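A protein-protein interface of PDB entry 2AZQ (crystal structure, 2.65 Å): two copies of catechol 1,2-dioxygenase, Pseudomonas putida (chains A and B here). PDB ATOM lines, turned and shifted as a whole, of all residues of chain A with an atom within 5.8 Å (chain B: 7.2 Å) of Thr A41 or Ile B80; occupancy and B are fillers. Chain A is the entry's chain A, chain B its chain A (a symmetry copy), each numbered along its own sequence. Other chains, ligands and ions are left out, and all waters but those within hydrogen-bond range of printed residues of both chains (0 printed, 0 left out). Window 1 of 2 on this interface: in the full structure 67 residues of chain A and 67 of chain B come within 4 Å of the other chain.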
ATOM      1  N   PHE A  14      22.838   3.175  11.792  1.00  0.00           N
ATOM      2  CA  PHE A  14      21.400   3.016  11.932  1.00  0.00           C
ATOM      3  C   PHE A  14      20.652   4.372  12.013  1.00  0.00           C
ATOM      4  O   PHE A  14      19.617   4.572  11.365  1.00  0.00           O
ATOM      5  CB  PHE A  14      21.113   2.139  13.156  1.00  0.00           C
ATOM      6  CG  PHE A  14      19.660   2.065  13.530  1.00  0.00           C
ATOM      7  CD1 PHE A  14      18.694   1.736  12.592  1.00  0.00           C
ATOM      8  CD2 PHE A  14      19.255   2.317  14.843  1.00  0.00           C
ATOM      9  CE1 PHE A  14      17.358   1.663  12.959  1.00  0.00           C
ATOM     10  CE2 PHE A  14      17.913   2.238  15.206  1.00  0.00           C
ATOM     11  CZ  PHE A  14      16.971   1.915  14.270  1.00  0.00           C
ATOM     12  N   PHE A  15      21.187   5.309  12.786  1.00  0.00           N
ATOM     13  CA  PHE A  15      20.565   6.617  12.923  1.00  0.00           C
ATOM     14  C   PHE A  15      20.639   7.312  11.597  1.00  0.00           C
ATOM     15  O   PHE A  15      19.745   8.057  11.235  1.00  0.00           O
ATOM     16  CB  PHE A  15      21.276   7.424  14.008  1.00  0.00           C
ATOM     17  CG  PHE A  15      20.989   6.927  15.392  1.00  0.00           C
ATOM     18  CD1 PHE A  15      21.902   7.099  16.417  1.00  0.00           C
ATOM     19  CD2 PHE A  15      19.805   6.253  15.665  1.00  0.00           C
ATOM     20  CE1 PHE A  15      21.636   6.592  17.693  1.00  0.00           C
ATOM     21  CE2 PHE A  15      19.538   5.751  16.937  1.00  0.00           C
ATOM     22  CZ  PHE A  15      20.450   5.918  17.943  1.00  0.00           C
ATOM     23  N   ARG A  36      20.864  14.418  14.432  1.00  0.00           N
ATOM     24  CA  ARG A  36      21.311  14.991  15.686  1.00  0.00           C
ATOM     25  C   ARG A  36      20.353  14.678  16.859  1.00  0.00           C
ATOM     26  O   ARG A  36      20.802  14.159  17.891  1.00  0.00           O
ATOM     27  CB  ARG A  36      21.494  16.506  15.480  1.00  0.00           C
ATOM     28  CG  ARG A  36      21.938  17.312  16.678  1.00  0.00           C
ATOM     29  CD  ARG A  36      23.164  16.769  17.330  1.00  0.00           C
ATOM     30  NE  ARG A  36      23.600  17.663  18.406  1.00  0.00           N
ATOM     31  CZ  ARG A  36      24.475  18.663  18.274  1.00  0.00           C
ATOM     32  NH1 ARG A  36      25.039  18.917  17.105  1.00  0.00           N
ATOM     33  NH2 ARG A  36      24.752  19.445  19.308  1.00  0.00           N
ATOM     34  N   VAL A  37      19.055  14.974  16.705  1.00  0.00           N
ATOM     35  CA  VAL A  37      18.087  14.699  17.775  1.00  0.00           C
ATOM     36  C   VAL A  37      18.184  13.240  18.232  1.00  0.00           C
ATOM     37  O   VAL A  37      17.996  12.936  19.422  1.00  0.00           O
ATOM     38  CB  VAL A  37      16.629  14.996  17.331  1.00  0.00           C
ATOM     39  CG1 VAL A  37      15.658  14.579  18.411  1.00  0.00           C
ATOM     40  CG2 VAL A  37      16.437  16.462  17.112  1.00  0.00           C
ATOM     41  N   LEU A  38      18.484  12.334  17.296  1.00  0.00           N
ATOM     42  CA  LEU A  38      18.617  10.918  17.651  1.00  0.00           C
ATOM     43  C   LEU A  38      19.909  10.546  18.407  1.00  0.00           C
ATOM     44  O   LEU A  38      19.858   9.748  19.331  1.00  0.00           O
ATOM     45  CB  LEU A  38      18.472  10.029  16.407  1.00  0.00           C
ATOM     46  CG  LEU A  38      17.080   9.903  15.771  1.00  0.00           C
ATOM     47  CD1 LEU A  38      17.224   9.215  14.401  1.00  0.00           C
ATOM     48  CD2 LEU A  38      16.125   9.148  16.703  1.00  0.00           C
ATOM     49  N   GLN A  39      21.051  11.124  18.018  1.00  0.00           N
ATOM     50  CA  GLN A  39      22.337  10.837  18.665  1.00  0.00           C
ATOM     51  C   GLN A  39      22.333  11.359  20.083  1.00  0.00           C
ATOM     52  O   GLN A  39      22.893  10.725  20.986  1.00  0.00           O
ATOM     53  CB  GLN A  39      23.500  11.522  17.959  1.00  0.00           C
ATOM     54  CG  GLN A  39      23.709  11.222  16.500  1.00  0.00           C
ATOM     55  CD  GLN A  39      24.924  11.968  15.977  1.00  0.00           C
ATOM     56  OE1 GLN A  39      26.033  11.804  16.498  1.00  0.00           O
ATOM     57  NE2 GLN A  39      24.725  12.803  14.968  1.00  0.00           N
ATOM     58  N   ASP A  40      21.741  12.540  20.267  1.00  0.00           N
ATOM     59  CA  ASP A  40      21.659  13.140  21.593  1.00  0.00           C
ATOM     60  C   ASP A  40      20.664  12.369  22.462  1.00  0.00           C
ATOM     61  O   ASP A  40      20.986  11.990  23.585  1.00  0.00           O
ATOM     62  CB  ASP A  40      21.225  14.606  21.516  1.00  0.00           C
ATOM     63  CG  ASP A  40      22.287  15.515  20.911  1.00  0.00           C
ATOM     64  OD1 ASP A  40      22.054  16.737  20.828  1.00  0.00           O
ATOM     65  OD2 ASP A  40      23.355  15.009  20.521  1.00  0.00           O
ATOM     66  N   THR A  41      19.461  12.121  21.951  1.00  0.00           N
ATOM     67  CA  THR A  41      18.476  11.395  22.739  1.00  0.00           C
ATOM     68  C   THR A  41      19.069  10.089  23.256  1.00  0.00           C
ATOM     69  O   THR A  41      18.909   9.733  24.427  1.00  0.00           O
ATOM     70  CB  THR A  41      17.200  11.136  21.913  1.00  0.00           C
ATOM     71  OG1 THR A  41      16.523  12.378  21.721  1.00  0.00           O
ATOM     72  CG2 THR A  41      16.257  10.183  22.637  1.00  0.00           C
ATOM     73  N   ALA A  42      19.778   9.392  22.381  1.00  0.00           N
ATOM     74  CA  ALA A  42      20.424   8.146  22.731  1.00  0.00           C
ATOM     75  C   ALA A  42      21.441   8.318  23.871  1.00  0.00           C
ATOM     76  O   ALA A  42      21.533   7.465  24.762  1.00  0.00           O
ATOM     77  CB  ALA A  42      21.110   7.579  21.511  1.00  0.00           C
ATOM     78  N   ARG A  43      22.212   9.409  23.839  1.00  0.00           N
ATOM     79  CA  ARG A  43      23.202   9.664  24.886  1.00  0.00           C
ATOM     80  C   ARG A  43      22.570   9.936  26.245  1.00  0.00           C
ATOM     81  O   ARG A  43      23.097   9.500  27.254  1.00  0.00           O
ATOM     82  CB  ARG A  43      24.100  10.838  24.530  1.00  0.00           C
ATOM     83  CG  ARG A  43      25.015  10.621  23.383  1.00  0.00           C
ATOM     84  CD  ARG A  43      25.564  11.958  22.873  1.00  0.00           C
ATOM     85  NE  ARG A  43      26.234  11.767  21.588  1.00  0.00           N
ATOM     86  CZ  ARG A  43      26.605  12.744  20.763  1.00  0.00           C
ATOM     87  NH1 ARG A  43      26.371  14.014  21.079  1.00  0.00           N
ATOM     88  NH2 ARG A  43      27.205  12.446  19.610  1.00  0.00           N
ATOM     89  N   LEU A  44      21.475  10.683  26.300  1.00  0.00           N
ATOM     90  CA  LEU A  44      20.856  10.889  27.604  1.00  0.00           C
ATOM     91  C   LEU A  44      20.551   9.501  28.150  1.00  0.00           C
ATOM     92  O   LEU A  44      20.940   9.145  29.255  1.00  0.00           O
ATOM     93  CB  LEU A  44      19.497  11.566  27.537  1.00  0.00           C
ATOM     94  CG  LEU A  44      19.019  12.935  27.147  1.00  0.00           C
ATOM     95  CD1 LEU A  44      17.551  12.885  27.428  1.00  0.00           C
ATOM     96  CD2 LEU A  44      19.644  14.043  27.962  1.00  0.00           C
ATOM     97  N   ILE A  45      19.791   8.743  27.368  1.00  0.00           N
ATOM     98  CA  ILE A  45      19.410   7.415  27.774  1.00  0.00           C
ATOM     99  C   ILE A  45      20.613   6.615  28.263  1.00  0.00           C
ATOM    100  O   ILE A  45      20.510   5.859  29.216  1.00  0.00           O
ATOM    101  CB  ILE A  45      18.717   6.680  26.615  1.00  0.00           C
ATOM    102  CG1 ILE A  45      17.425   7.416  26.255  1.00  0.00           C
ATOM    103  CG2 ILE A  45      18.464   5.228  26.990  1.00  0.00           C
ATOM    104  CD1 ILE A  45      16.827   6.986  24.930  1.00  0.00           C
ATOM    105  N   GLU A  46      21.760   6.781  27.628  1.00  0.00           N
ATOM    106  CA  GLU A  46      22.929   6.037  28.062  1.00  0.00           C
ATOM    107  C   GLU A  46      23.704   6.684  29.203  1.00  0.00           C
ATOM    108  O   GLU A  46      24.334   5.989  29.988  1.00  0.00           O
ATOM    109  CB  GLU A  46      23.856   5.769  26.871  1.00  0.00           C
ATOM    110  CG  GLU A  46      23.402   4.596  25.985  1.00  0.00           C
ATOM    111  CD  GLU A  46      24.202   4.477  24.702  1.00  0.00           C
ATOM    112  OE1 GLU A  46      24.026   3.474  23.974  1.00  0.00           O
ATOM    113  OE2 GLU A  46      24.999   5.393  24.412  1.00  0.00           O
ATOM    114  N   PHE A  55      11.211   6.022  30.045  1.00  0.00           N
ATOM    115  CA  PHE A  55      11.099   6.347  28.637  1.00  0.00           C
ATOM    116  C   PHE A  55       9.671   6.350  28.155  1.00  0.00           C
ATOM    117  O   PHE A  55       9.271   7.278  27.439  1.00  0.00           O
ATOM    118  CB  PHE A  55      11.877   5.366  27.776  1.00  0.00           C
ATOM    119  CG  PHE A  55      11.801   5.684  26.338  1.00  0.00           C
ATOM    120  CD1 PHE A  55      12.708   6.542  25.766  1.00  0.00           C
ATOM    121  CD2 PHE A  55      10.749   5.209  25.563  1.00  0.00           C
ATOM    122  CE1 PHE A  55      12.577   6.931  24.444  1.00  0.00           C
ATOM    123  CE2 PHE A  55      10.609   5.598  24.240  1.00  0.00           C
ATOM    124  CZ  PHE A  55      11.535   6.465  23.686  1.00  0.00           C
ATOM    125  N   ASP B  40      21.217  20.288  26.478  1.00  0.00           N
ATOM    126  CA  ASP B  40      21.323  19.689  25.154  1.00  0.00           C
ATOM    127  C   ASP B  40      20.419  20.428  24.165  1.00  0.00           C
ATOM    128  O   ASP B  40      20.868  20.819  23.090  1.00  0.00           O
ATOM    129  CB  ASP B  40      20.932  18.209  25.179  1.00  0.00           C
ATOM    130  CG  ASP B  40      21.940  17.335  25.915  1.00  0.00           C
ATOM    131  OD1 ASP B  40      21.740  16.106  25.970  1.00  0.00           O
ATOM    132  OD2 ASP B  40      22.933  17.876  26.434  1.00  0.00           O
ATOM    133  N   LEU B  74       5.756   7.619  16.467  1.00  0.00           N
ATOM    134  CA  LEU B  74       6.926   8.325  16.001  1.00  0.00           C
ATOM    135  C   LEU B  74       8.215   7.742  16.607  1.00  0.00           C
ATOM    136  O   LEU B  74       9.215   7.619  15.899  1.00  0.00           O
ATOM    137  CB  LEU B  74       6.827   9.799  16.363  1.00  0.00           C
ATOM    138  CG  LEU B  74       7.955  10.656  15.800  1.00  0.00           C
ATOM    139  CD1 LEU B  74       8.028  10.523  14.255  1.00  0.00           C
ATOM    140  CD2 LEU B  74       7.683  12.073  16.242  1.00  0.00           C
ATOM    141  N   ALA B  75       8.220   7.387  17.894  1.00  0.00           N
ATOM    142  CA  ALA B  75       9.441   6.821  18.496  1.00  0.00           C
ATOM    143  C   ALA B  75       9.755   5.553  17.704  1.00  0.00           C
ATOM    144  O   ALA B  75      10.908   5.198  17.466  1.00  0.00           O
ATOM    145  CB  ALA B  75       9.223   6.491  20.011  1.00  0.00           C
ATOM    146  N   ALA B  76       8.690   4.885  17.277  1.00  0.00           N
ATOM    147  CA  ALA B  76       8.806   3.666  16.495  1.00  0.00           C
ATOM    148  C   ALA B  76       9.369   3.952  15.090  1.00  0.00           C
ATOM    149  O   ALA B  76      10.232   3.237  14.587  1.00  0.00           O
ATOM    150  CB  ALA B  76       7.448   3.009  16.385  1.00  0.00           C
ATOM    151  N   GLY B  77       8.873   5.010  14.466  1.00  0.00           N
ATOM    152  CA  GLY B  77       9.329   5.346  13.139  1.00  0.00           C
ATOM    153  C   GLY B  77      10.740   5.892  13.117  1.00  0.00           C
ATOM    154  O   GLY B  77      11.451   5.730  12.118  1.00  0.00           O
ATOM    155  N   LEU B  78      11.163   6.544  14.198  1.00  0.00           N
ATOM    156  CA  LEU B  78      12.512   7.083  14.221  1.00  0.00           C
ATOM    157  C   LEU B  78      13.535   6.045  14.696  1.00  0.00           C
ATOM    158  O   LEU B  78      14.727   6.337  14.847  1.00  0.00           O
ATOM    159  CB  LEU B  78      12.572   8.366  15.058  1.00  0.00           C
ATOM    160  CG  LEU B  78      11.621   9.466  14.579  1.00  0.00           C
ATOM    161  CD1 LEU B  78      12.196  10.793  14.976  1.00  0.00           C
ATOM    162  CD2 LEU B  78      11.466   9.471  13.083  1.00  0.00           C
ATOM    163  N   GLY B  79      13.064   4.821  14.906  1.00  0.00           N
ATOM    164  CA  GLY B  79      13.963   3.759  15.294  1.00  0.00           C
ATOM    165  C   GLY B  79      14.345   3.776  16.745  1.00  0.00           C
ATOM    166  O   GLY B  79      15.207   2.995  17.171  1.00  0.00           O
ATOM    167  N   ILE B  80      13.702   4.665  17.500  1.00  0.00           N
ATOM    168  CA  ILE B  80      13.930   4.802  18.938  1.00  0.00           C
ATOM    169  C   ILE B  80      13.466   3.530  19.684  1.00  0.00           C
ATOM    170  O   ILE B  80      14.114   3.055  20.611  1.00  0.00           O
ATOM    171  CB  ILE B  80      13.189   6.087  19.473  1.00  0.00           C
ATOM    172  CG1 ILE B  80      14.066   7.336  19.328  1.00  0.00           C
ATOM    173  CG2 ILE B  80      12.757   5.887  20.907  1.00  0.00           C
ATOM    174  CD1 ILE B  80      15.301   7.290  20.222  1.00  0.00           C
ATOM    175  N   GLU B  81      12.355   2.952  19.263  1.00  0.00           N
ATOM    176  CA  GLU B  81      11.901   1.754  19.943  1.00  0.00           C
ATOM    177  C   GLU B  81      12.865   0.587  19.658  1.00  0.00           C
ATOM    178  O   GLU B  81      13.244  -0.166  20.578  1.00  0.00           O
ATOM    179  CB  GLU B  81      10.468   1.408  19.525  1.00  0.00           C
ATOM    180  CG  GLU B  81       9.782   0.566  20.543  1.00  0.00           C
ATOM    181  CD  GLU B  81       8.308   0.428  20.295  1.00  0.00           C
ATOM    182  OE1 GLU B  81       7.662  -0.389  20.991  1.00  0.00           O
ATOM    183  OE2 GLU B  81       7.785   1.141  19.412  1.00  0.00           O
ATOM    184  N   HIS B  82      13.273   0.425  18.399  1.00  0.00           N
ATOM    185  CA  HIS B  82      14.218  -0.657  18.097  1.00  0.00           C
ATOM    186  C   HIS B  82      15.499  -0.471  18.927  1.00  0.00           C
ATOM    187  O   HIS B  82      16.020  -1.447  19.528  1.00  0.00           O
ATOM    188  CB  HIS B  82      14.567  -0.694  16.605  1.00  0.00           C
ATOM    189  CG  HIS B  82      15.608  -1.716  16.247  1.00  0.00           C
ATOM    190  ND1 HIS B  82      15.492  -3.047  16.572  1.00  0.00           N
ATOM    191  CD2 HIS B  82      16.763  -1.606  15.553  1.00  0.00           C
ATOM    192  CE1 HIS B  82      16.525  -3.714  16.094  1.00  0.00           C
ATOM    193  NE2 HIS B  82      17.310  -2.863  15.470  1.00  0.00           N
ATOM    194  N   PHE B  83      15.990   0.777  18.960  1.00  0.00           N
ATOM    195  CA  PHE B  83      17.195   1.110  19.702  1.00  0.00           C
ATOM    196  C   PHE B  83      17.127   0.651  21.165  1.00  0.00           C
ATOM    197  O   PHE B  83      18.137   0.211  21.737  1.00  0.00           O
ATOM    198  CB  PHE B  83      17.457   2.614  19.672  1.00  0.00           C
ATOM    199  CG  PHE B  83      18.571   3.035  20.592  1.00  0.00           C
ATOM    200  CD1 PHE B  83      19.897   2.727  20.292  1.00  0.00           C
ATOM    201  CD2 PHE B  83      18.283   3.638  21.821  1.00  0.00           C
ATOM    202  CE1 PHE B  83      20.919   3.003  21.198  1.00  0.00           C
ATOM    203  CE2 PHE B  83      19.308   3.922  22.736  1.00  0.00           C
ATOM    204  CZ  PHE B  83      20.629   3.600  22.419  1.00  0.00           C
ATOM    205  N   LEU B  84      15.957   0.775  21.786  1.00  0.00           N
ATOM    206  CA  LEU B  84      15.855   0.328  23.162  1.00  0.00           C
ATOM    207  C   LEU B  84      16.069  -1.178  23.257  1.00  0.00           C
ATOM    208  O   LEU B  84      16.767  -1.633  24.162  1.00  0.00           O
ATOM    209  CB  LEU B  84      14.506   0.703  23.788  1.00  0.00           C
ATOM    210  CG  LEU B  84      14.268   2.181  24.050  1.00  0.00           C
ATOM    211  CD1 LEU B  84      12.815   2.410  24.425  1.00  0.00           C
ATOM    212  CD2 LEU B  84      15.244   2.667  25.154  1.00  0.00           C
ATOM    213  N   ASP B  85      15.495  -1.958  22.340  1.00  0.00           N
ATOM    214  CA  ASP B  85      15.698  -3.404  22.422  1.00  0.00           C
ATOM    215  C   ASP B  85      17.183  -3.730  22.209  1.00  0.00           C
ATOM    216  O   ASP B  85      17.701  -4.703  22.776  1.00  0.00           O
ATOM    217  CB  ASP B  85      14.881  -4.191  21.379  1.00  0.00           C
ATOM    218  CG  ASP B  85      13.377  -4.028  21.526  1.00  0.00           C
ATOM    219  OD1 ASP B  85      12.846  -3.984  22.648  1.00  0.00           O
ATOM    220  OD2 ASP B  85      12.711  -3.989  20.485  1.00  0.00           O
ATOM    221  N   LEU B  86      17.867  -2.925  21.395  1.00  0.00           N
ATOM    222  CA  LEU B  86      19.275  -3.184  21.149  1.00  0.00           C
ATOM    223  C   LEU B  86      20.070  -3.022  22.412  1.00  0.00           C
ATOM    224  O   LEU B  86      20.958  -3.827  22.715  1.00  0.00           O
ATOM    225  CB  LEU B  86      19.843  -2.254  20.070  1.00  0.00           C
ATOM    226  CG  LEU B  86      19.355  -2.582  18.651  1.00  0.00           C
ATOM    227  CD1 LEU B  86      20.080  -1.739  17.626  1.00  0.00           C
ATOM    228  CD2 LEU B  86      19.576  -4.068  18.377  1.00  0.00           C
ATOM    229  N   ILE B 105      10.388  -4.738  19.212  1.00  0.00           N
ATOM    230  CA  ILE B 105       9.432  -3.747  19.649  1.00  0.00           C
ATOM    231  C   ILE B 105       8.005  -4.195  19.806  1.00  0.00           C
ATOM    232  O   ILE B 105       7.497  -5.000  19.036  1.00  0.00           O
ATOM    233  CB  ILE B 105       9.453  -2.480  18.781  1.00  0.00           C
ATOM    234  CG1 ILE B 105       8.738  -2.717  17.446  1.00  0.00           C
ATOM    235  CG2 ILE B 105      10.902  -1.998  18.642  1.00  0.00           C
ATOM    236  CD1 ILE B 105       8.474  -1.446  16.665  1.00  0.00           C
ATOM    237  N   ALA B 251       9.695   0.701  11.125  1.00  0.00           N
ATOM    238  CA  ALA B 251       9.910   0.677  12.571  1.00  0.00           C
ATOM    239  C   ALA B 251      11.018  -0.286  12.911  1.00  0.00           C
ATOM    240  O   ALA B 251      11.245  -0.581  14.084  1.00  0.00           O
ATOM    241  CB  ALA B 251       8.639   0.273  13.317  1.00  0.00           C
ATOM    242  N   TYR B 252      11.684  -0.794  11.877  1.00  0.00           N
ATOM    243  CA  TYR B 252      12.819  -1.706  12.009  1.00  0.00           C
ATOM    244  C   TYR B 252      12.670  -2.817  13.031  1.00  0.00           C
ATOM    245  O   TYR B 252      13.606  -3.084  13.777  1.00  0.00           O
ATOM    246  CB  TYR B 252      14.072  -0.913  12.369  1.00  0.00           C
ATOM    247  CG  TYR B 252      14.271   0.340  11.548  1.00  0.00           C
ATOM    248  CD1 TYR B 252      13.688   1.543  11.917  1.00  0.00           C
ATOM    249  CD2 TYR B 252      15.013   0.308  10.381  1.00  0.00           C
ATOM    250  CE1 TYR B 252      13.849   2.681  11.132  1.00  0.00           C
ATOM    251  CE2 TYR B 252      15.181   1.421   9.596  1.00  0.00           C
ATOM    252  CZ  TYR B 252      14.607   2.604   9.960  1.00  0.00           C
ATOM    253  OH  TYR B 252      14.795   3.706   9.142  1.00  0.00           O
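Of the printed residues of chain B, Leu A38 touches Leu B78 and Ile B80.
Thr A41 touches just one residue of chain B: Ile B80.
Of the printed residues of chain B, Leu A44 touches Asp B40.
Of chain A, only Leu A38, Thr A41 and Phe A55 come within 4 Å of Ile B80.
Of the printed residues of chain A, Phe B83 touches Glu A46 (3.7 Å).
The nearest residue of chain A that does not touch Ile B80 is Ile A45 (5.0 Å).
The nearest printed residue of chain B that does not touch Phe A55 is Ala B75 (4.3 Å).
Among the printed residues, merely in contact across the chains: Phe A14 with Gly B79, Phe A14 with His B82, Phe A14 with Tyr B252, Leu A38 with Leu B78, Leu A38 with Ile B80, Thr A41 with Ile B80, Leu A44 with Asp B40, Glu A46 with Phe B83, Phe A55 with Ile B80 and Phe A55 with Leu B84.
Position printed for both chains: 40.
Hydrophobic or aromatic side chains of chain B that line the printed part of chain A: Leu B78, Ile B80, His B82, Phe B83, Leu B84 and Tyr B252.
Of the 14 printed residues of chain A, 6 touch a printed residue of chain B.
Among the printed residues, 10 pairs touch across the chains.
Among the printed residues, no Asp or Glu carboxylate lies within 4 Å of a Lys or Arg side-chain nitrogen of the other chain.
O of Val A37 is in hydrogen-bond range of OG1 of Thr A41 (2.8 Å).
The backbone carbonyl oxygen (O) of Ala B75 sits at hydrogen-bond distance from the backbone NH (N) of Ile B80.
A ring nitrogen (ND1) of His B82 sits at hydrogen-bond distance from the backbone carbonyl oxygen of Tyr B252 (3.4 Å).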
